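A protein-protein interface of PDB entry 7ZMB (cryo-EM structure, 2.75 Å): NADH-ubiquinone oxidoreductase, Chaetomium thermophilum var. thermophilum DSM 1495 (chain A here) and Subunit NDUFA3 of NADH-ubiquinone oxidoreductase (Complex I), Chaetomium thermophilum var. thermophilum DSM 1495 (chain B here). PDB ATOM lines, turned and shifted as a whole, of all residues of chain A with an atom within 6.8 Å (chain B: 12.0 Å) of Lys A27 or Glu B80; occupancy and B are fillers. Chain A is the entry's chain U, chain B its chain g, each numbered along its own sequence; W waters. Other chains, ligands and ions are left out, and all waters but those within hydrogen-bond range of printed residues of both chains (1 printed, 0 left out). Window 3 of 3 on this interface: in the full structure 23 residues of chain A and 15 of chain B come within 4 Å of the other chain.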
ATOM      1  N   LYS A  25     -22.014   8.748  -1.323  1.00  0.00           N
ATOM      2  CA  LYS A  25     -22.383   7.519  -2.066  1.00  0.00           C
ATOM      3  C   LYS A  25     -22.150   7.701  -3.565  1.00  0.00           C
ATOM      4  O   LYS A  25     -22.370   8.815  -4.063  1.00  0.00           O
ATOM      5  CB  LYS A  25     -23.847   7.164  -1.789  1.00  0.00           C
ATOM      6  CG  LYS A  25     -24.166   6.875  -0.330  1.00  0.00           C
ATOM      7  CD  LYS A  25     -25.639   6.658  -0.063  1.00  0.00           C
ATOM      8  CE  LYS A  25     -25.933   6.391   1.398  1.00  0.00           C
ATOM      9  NZ  LYS A  25     -25.407   7.472   2.265  1.00  0.00           N
ATOM     10  N   VAL A  26     -21.677   6.650  -4.240  1.00  0.00           N
ATOM     11  CA  VAL A  26     -21.540   6.697  -5.724  1.00  0.00           C
ATOM     12  C   VAL A  26     -22.208   5.443  -6.280  1.00  0.00           C
ATOM     13  O   VAL A  26     -21.816   4.356  -5.868  1.00  0.00           O
ATOM     14  CB  VAL A  26     -20.068   6.819  -6.165  1.00  0.00           C
ATOM     15  CG1 VAL A  26     -19.167   5.760  -5.553  1.00  0.00           C
ATOM     16  CG2 VAL A  26     -19.906   6.882  -7.672  1.00  0.00           C
ATOM     17  N   LYS A  27     -23.165   5.580  -7.192  1.00  0.00           N
ATOM     18  CA  LYS A  27     -23.757   4.384  -7.842  1.00  0.00           C
ATOM     19  C   LYS A  27     -22.649   3.679  -8.638  1.00  0.00           C
ATOM     20  O   LYS A  27     -22.057   4.340  -9.505  1.00  0.00           O
ATOM     21  CB  LYS A  27     -24.919   4.794  -8.748  1.00  0.00           C
ATOM     22  CG  LYS A  27     -25.962   5.700  -8.110  1.00  0.00           C
ATOM     23  CD  LYS A  27     -26.968   6.230  -9.109  1.00  0.00           C
ATOM     24  CE  LYS A  27     -27.860   7.310  -8.539  1.00  0.00           C
ATOM     25  NZ  LYS A  27     -27.086   8.510  -8.142  1.00  0.00           N
ATOM     26  N   GLU A  28     -22.382   2.394  -8.371  1.00  0.00           N
ATOM     27  CA  GLU A  28     -21.263   1.714  -9.070  1.00  0.00           C
ATOM     28  C   GLU A  28     -21.597   1.446 -10.543  1.00  0.00           C
ATOM     29  O   GLU A  28     -22.781   1.376 -10.885  1.00  0.00           O
ATOM     30  CB  GLU A  28     -20.898   0.417  -8.357  1.00  0.00           C
ATOM     31  CG  GLU A  28     -20.602   0.573  -6.876  1.00  0.00           C
ATOM     32  CD  GLU A  28     -19.263   1.187  -6.505  1.00  0.00           C
ATOM     33  OE1 GLU A  28     -18.451   1.452  -7.411  1.00  0.00           O
ATOM     34  OE2 GLU A  28     -19.035   1.398  -5.302  1.00  0.00           O
ATOM     35  N   ILE A  29     -20.573   1.329 -11.384  1.00  0.00           N
ATOM     36  CA  ILE A  29     -20.773   0.991 -12.824  1.00  0.00           C
ATOM     37  C   ILE A  29     -21.457  -0.365 -12.882  1.00  0.00           C
ATOM     38  O   ILE A  29     -21.024  -1.272 -12.157  1.00  0.00           O
ATOM     39  CB  ILE A  29     -19.408   0.937 -13.544  1.00  0.00           C
ATOM     40  CG1 ILE A  29     -18.705   2.295 -13.566  1.00  0.00           C
ATOM     41  CG2 ILE A  29     -19.548   0.347 -14.939  1.00  0.00           C
ATOM     42  CD1 ILE A  29     -19.485   3.358 -14.280  1.00  0.00           C
ATOM     43  N   GLY A  30     -22.465  -0.501 -13.735  1.00  0.00           N
ATOM     44  CA  GLY A  30     -23.224  -1.757 -13.829  1.00  0.00           C
ATOM     45  C   GLY A  30     -22.875  -2.571 -15.045  1.00  0.00           C
ATOM     46  O   GLY A  30     -23.485  -3.624 -15.225  1.00  0.00           O
ATOM     47  N   ARG A  74     -14.473   8.219  -6.749  1.00  0.00           N
ATOM     48  CA  ARG A  74     -15.884   8.552  -7.074  1.00  0.00           C
ATOM     49  C   ARG A  74     -15.905   9.309  -8.399  1.00  0.00           C
ATOM     50  O   ARG A  74     -16.813   9.062  -9.203  1.00  0.00           O
ATOM     51  CB  ARG A  74     -16.505   9.367  -5.942  1.00  0.00           C
ATOM     52  CG  ARG A  74     -16.711   8.581  -4.660  1.00  0.00           C
ATOM     53  CD  ARG A  74     -17.616   9.263  -3.653  1.00  0.00           C
ATOM     54  NE  ARG A  74     -17.129  10.569  -3.239  1.00  0.00           N
ATOM     55  CZ  ARG A  74     -16.284  10.785  -2.242  1.00  0.00           C
ATOM     56  NH1 ARG A  74     -15.807   9.773  -1.541  1.00  0.00           N
ATOM     57  NH2 ARG A  74     -15.918  12.017  -1.948  1.00  0.00           N
ATOM     58  N   THR A  77     -15.503   6.894 -11.348  1.00  0.00           N
ATOM     59  CA  THR A  77     -16.727   6.081 -11.525  1.00  0.00           C
ATOM     60  C   THR A  77     -17.757   6.947 -12.241  1.00  0.00           C
ATOM     61  O   THR A  77     -18.373   6.444 -13.191  1.00  0.00           O
ATOM     62  CB  THR A  77     -17.213   5.554 -10.170  1.00  0.00           C
ATOM     63  OG1 THR A  77     -16.214   4.663  -9.676  1.00  0.00           O
ATOM     64  CG2 THR A  77     -18.544   4.839 -10.248  1.00  0.00           C
ATOM     65  N   ARG A  78     -17.911   8.199 -11.813  1.00  0.00           N
ATOM     66  CA  ARG A  78     -18.898   9.116 -12.430  1.00  0.00           C
ATOM     67  C   ARG A  78     -18.492   9.400 -13.876  1.00  0.00           C
ATOM     68  O   ARG A  78     -19.380   9.354 -14.749  1.00  0.00           O
ATOM     69  CB  ARG A  78     -19.049  10.376 -11.573  1.00  0.00           C
ATOM     70  CG  ARG A  78     -20.068  10.222 -10.454  1.00  0.00           C
ATOM     71  CD  ARG A  78     -20.322  11.519  -9.718  1.00  0.00           C
ATOM     72  NE  ARG A  78     -19.171  11.936  -8.935  1.00  0.00           N
ATOM     73  CZ  ARG A  78     -19.013  11.693  -7.641  1.00  0.00           C
ATOM     74  NH1 ARG A  78     -19.944  11.041  -6.966  1.00  0.00           N
ATOM     75  NH2 ARG A  78     -17.927  12.116  -7.024  1.00  0.00           N
ATOM     76  N   ARG A  81     -19.208   6.573 -16.050  1.00  0.00           N
ATOM     77  CA  ARG A  81     -20.657   6.296 -16.236  1.00  0.00           C
ATOM     78  C   ARG A  81     -21.153   7.220 -17.346  1.00  0.00           C
ATOM     79  O   ARG A  81     -22.048   6.810 -18.089  1.00  0.00           O
ATOM     80  CB  ARG A  81     -21.411   6.611 -14.943  1.00  0.00           C
ATOM     81  CG  ARG A  81     -22.914   6.390 -14.983  1.00  0.00           C
ATOM     82  CD  ARG A  81     -23.508   7.124 -13.798  1.00  0.00           C
ATOM     83  NE  ARG A  81     -22.789   6.823 -12.569  1.00  0.00           N
ATOM     84  CZ  ARG A  81     -23.011   7.417 -11.403  1.00  0.00           C
ATOM     85  NH1 ARG A  81     -22.306   7.074 -10.339  1.00  0.00           N
ATOM     86  NH2 ARG A  81     -23.935   8.355 -11.304  1.00  0.00           N
ATOM     87  N   LYS B  73     -11.343  19.999 -12.148  1.00  0.00           N
ATOM     88  CA  LYS B  73     -12.673  20.399 -11.713  1.00  0.00           C
ATOM     89  C   LYS B  73     -13.699  19.689 -12.582  1.00  0.00           C
ATOM     90  O   LYS B  73     -13.586  19.695 -13.812  1.00  0.00           O
ATOM     91  CB  LYS B  73     -12.858  21.915 -11.800  1.00  0.00           C
ATOM     92  CG  LYS B  73     -11.822  22.711 -11.023  1.00  0.00           C
ATOM     93  CD  LYS B  73     -12.282  24.142 -10.796  1.00  0.00           C
ATOM     94  CE  LYS B  73     -12.772  24.780 -12.086  1.00  0.00           C
ATOM     95  NZ  LYS B  73     -11.717  24.790 -13.136  1.00  0.00           N
ATOM     96  N   GLY B  74     -14.675  19.034 -11.947  1.00  0.00           N
ATOM     97  CA  GLY B  74     -15.669  18.253 -12.709  1.00  0.00           C
ATOM     98  C   GLY B  74     -15.856  16.865 -12.139  1.00  0.00           C
ATOM     99  O   GLY B  74     -14.891  16.357 -11.559  1.00  0.00           O
ATOM    100  N   TYR B  75     -17.040  16.273 -12.313  1.00  0.00           N
ATOM    101  CA  TYR B  75     -17.371  14.919 -11.786  1.00  0.00           C
ATOM    102  C   TYR B  75     -17.322  14.900 -10.250  1.00  0.00           C
ATOM    103  O   TYR B  75     -17.074  13.836  -9.661  1.00  0.00           O
ATOM    104  CB  TYR B  75     -16.588  13.832 -12.520  1.00  0.00           C
ATOM    105  CG  TYR B  75     -16.852  13.755 -14.001  1.00  0.00           C
ATOM    106  CD1 TYR B  75     -18.063  13.294 -14.489  1.00  0.00           C
ATOM    107  CD2 TYR B  75     -15.889  14.137 -14.917  1.00  0.00           C
ATOM    108  CE1 TYR B  75     -18.309  13.214 -15.849  1.00  0.00           C
ATOM    109  CE2 TYR B  75     -16.120  14.071 -16.281  1.00  0.00           C
ATOM    110  CZ  TYR B  75     -17.334  13.602 -16.748  1.00  0.00           C
ATOM    111  OH  TYR B  75     -17.569  13.532 -18.091  1.00  0.00           O
ATOM    112  N   ASP B  76     -17.662  16.017  -9.605  1.00  0.00           N
ATOM    113  CA  ASP B  76     -17.581  16.075  -8.120  1.00  0.00           C
ATOM    114  C   ASP B  76     -18.819  15.417  -7.494  1.00  0.00           C
ATOM    115  O   ASP B  76     -19.677  14.952  -8.250  1.00  0.00           O
ATOM    116  CB  ASP B  76     -17.364  17.508  -7.627  1.00  0.00           C
ATOM    117  CG  ASP B  76     -15.978  18.041  -7.942  1.00  0.00           C
ATOM    118  OD1 ASP B  76     -15.149  17.257  -8.446  1.00  0.00           O
ATOM    119  OD2 ASP B  76     -15.738  19.236  -7.678  1.00  0.00           O
ATOM    120  N   ASP B  77     -18.909  15.383  -6.163  1.00  0.00           N
ATOM    121  CA  ASP B  77     -20.008  14.656  -5.460  1.00  0.00           C
ATOM    122  C   ASP B  77     -21.388  15.223  -5.805  1.00  0.00           C
ATOM    123  O   ASP B  77     -22.333  14.428  -5.885  1.00  0.00           O
ATOM    124  CB  ASP B  77     -19.752  14.572  -3.954  1.00  0.00           C
ATOM    125  CG  ASP B  77     -18.478  13.827  -3.607  1.00  0.00           C
ATOM    126  OD1 ASP B  77     -18.076  12.963  -4.404  1.00  0.00           O
ATOM    127  OD2 ASP B  77     -17.893  14.126  -2.552  1.00  0.00           O
ATOM    128  N   ASP B  78     -21.500  16.541  -5.986  1.00  0.00           N
ATOM    129  CA  ASP B  78     -22.802  17.187  -6.310  1.00  0.00           C
ATOM    130  C   ASP B  78     -23.347  16.627  -7.630  1.00  0.00           C
ATOM    131  O   ASP B  78     -24.579  16.483  -7.738  1.00  0.00           O
ATOM    132  CB  ASP B  78     -22.683  18.714  -6.335  1.00  0.00           C
ATOM    133  CG  ASP B  78     -21.713  19.247  -7.378  1.00  0.00           C
ATOM    134  OD1 ASP B  78     -20.680  18.590  -7.611  1.00  0.00           O
ATOM    135  OD2 ASP B  78     -22.005  20.313  -7.954  1.00  0.00           O
ATOM    136  N   THR B  79     -22.472  16.321  -8.589  1.00  0.00           N
ATOM    137  CA  THR B  79     -22.900  15.835  -9.932  1.00  0.00           C
ATOM    138  C   THR B  79     -23.498  14.425  -9.856  1.00  0.00           C
ATOM    139  O   THR B  79     -24.106  14.007 -10.857  1.00  0.00           O
ATOM    140  CB  THR B  79     -21.732  15.876 -10.924  1.00  0.00           C
ATOM    141  OG1 THR B  79     -20.879  14.762 -10.663  1.00  0.00           O
ATOM    142  CG2 THR B  79     -20.941  17.162 -10.855  1.00  0.00           C
ATOM    143  N   GLU B  80     -23.341  13.719  -8.730  1.00  0.00           N
ATOM    144  CA  GLU B  80     -23.802  12.307  -8.629  1.00  0.00           C
ATOM    145  C   GLU B  80     -25.309  12.216  -8.899  1.00  0.00           C
ATOM    146  O   GLU B  80     -25.719  11.288  -9.625  1.00  0.00           O
ATOM    147  CB  GLU B  80     -23.516  11.782  -7.221  1.00  0.00           C
ATOM    148  CG  GLU B  80     -24.070  10.396  -6.953  1.00  0.00           C
ATOM    149  CD  GLU B  80     -23.334   9.279  -7.666  1.00  0.00           C
ATOM    150  OE1 GLU B  80     -22.101   9.359  -7.767  1.00  0.00           O
ATOM    151  OE2 GLU B  80     -23.999   8.338  -8.129  1.00  0.00           O
ATOM    152  N   ASP B  81     -26.095  13.150  -8.359  1.00  0.00           N
ATOM    153  CA  ASP B  81     -27.562  13.158  -8.606  1.00  0.00           C
ATOM    154  C   ASP B  81     -27.865  14.033  -9.829  1.00  0.00           C
ATOM    155  O   ASP B  81     -27.751  13.501 -10.951  1.00  0.00           O
ATOM    156  CB  ASP B  81     -28.337  13.615  -7.367  1.00  0.00           C
HETATM  157  O   HOH W   1     -15.620  13.666  -6.588  1.00  0.00           O
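Printed residues of chain B that touch a printed residue of chain A: Tyr B75, Asp B76, Asp B77, Thr B79 and Glu B80. Hydrophobic or aromatic side chains of chain B within 4 Å of the printed part of chain A: Tyr B75. Of the 10 printed residues of chain A, 6 touch a printed residue of chain B. Among the printed residues, 10 pairs touch across the chains.
Lys A27 touches one residue of chain B. Val A26 touches one residue of chain B. No residue of chain B comes within 4 Å of Glu A28. No residue of chain B comes within 4 Å of Ile A29. No residue of chain B comes within 4 Å of Thr A77. Arg A78 touches five residues of chain B. Printed residues of chain B within 4 Å of Lys A25: Glu B80. Of the printed residues of chain B, Arg A81 touches Glu B80. Of the printed residues of chain A, Asp B76 touches Arg A78 (3.1 Å). The nearest residue of chain B that does not touch Lys A27 is Asp B81 (4.7 Å).
Among the printed residues, pairs that only touch across the chains: Lys A25 with Glu B80 (3.7 Å), Val A26 with Glu B80 (3.3 Å) and Arg A78 with Thr B79 (3.4 Å).
Water W1 lies within hydrogen-bond range of the guanidinium group (NH2) of Arg A78 (2.8 Å), the side-chain carboxylate (OD1) of Asp B77 (3.4 Å) and the backbone carbonyl oxygen (O) of Tyr B75 (3.4 Å).
The guanidinium group (NH1) of Arg A81 is in hydrogen-bond range of the backbone carbonyl oxygen (O) of Lys A27, at 2.9 Å. The backbone carbonyl oxygen (O) of Asp B76 is in hydrogen-bond range of the side-chain hydroxyl (OG1) of Thr B79 (2.7 Å).
The guanidinium group (NH2) of Arg A78 is in salt-bridge range of the side-chain carboxylate (OD1) of Asp B77 (2.8 Å). The guanidinium group of Arg A78 lies within salt-bridge range of the side-chain carboxylate of Glu B80 (2.9 Å). The side-chain carboxylate (OE2) of Glu B80 lies within salt-bridge range of the side-chain amino group (NZ) of Lys A27 (3.1 Å). The guanidinium group (NE) of Arg A74 is in salt-bridge range of the side-chain carboxylate (OD1) of Asp B77 (2.8 Å). The guanidinium group of Arg A78 lies within hydrogen-bond range of the backbone carbonyl oxygen of Asp B76 (3.1 Å). The backbone carbonyl oxygen of Tyr B75 is in hydrogen-bond range of the guanidinium group of Arg A78 (2.9 Å). The guanidinium group (NH1) of Arg A81 is in salt-bridge range of the side-chain carboxylate (OE2) of Glu B80, at 3.1 Å.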
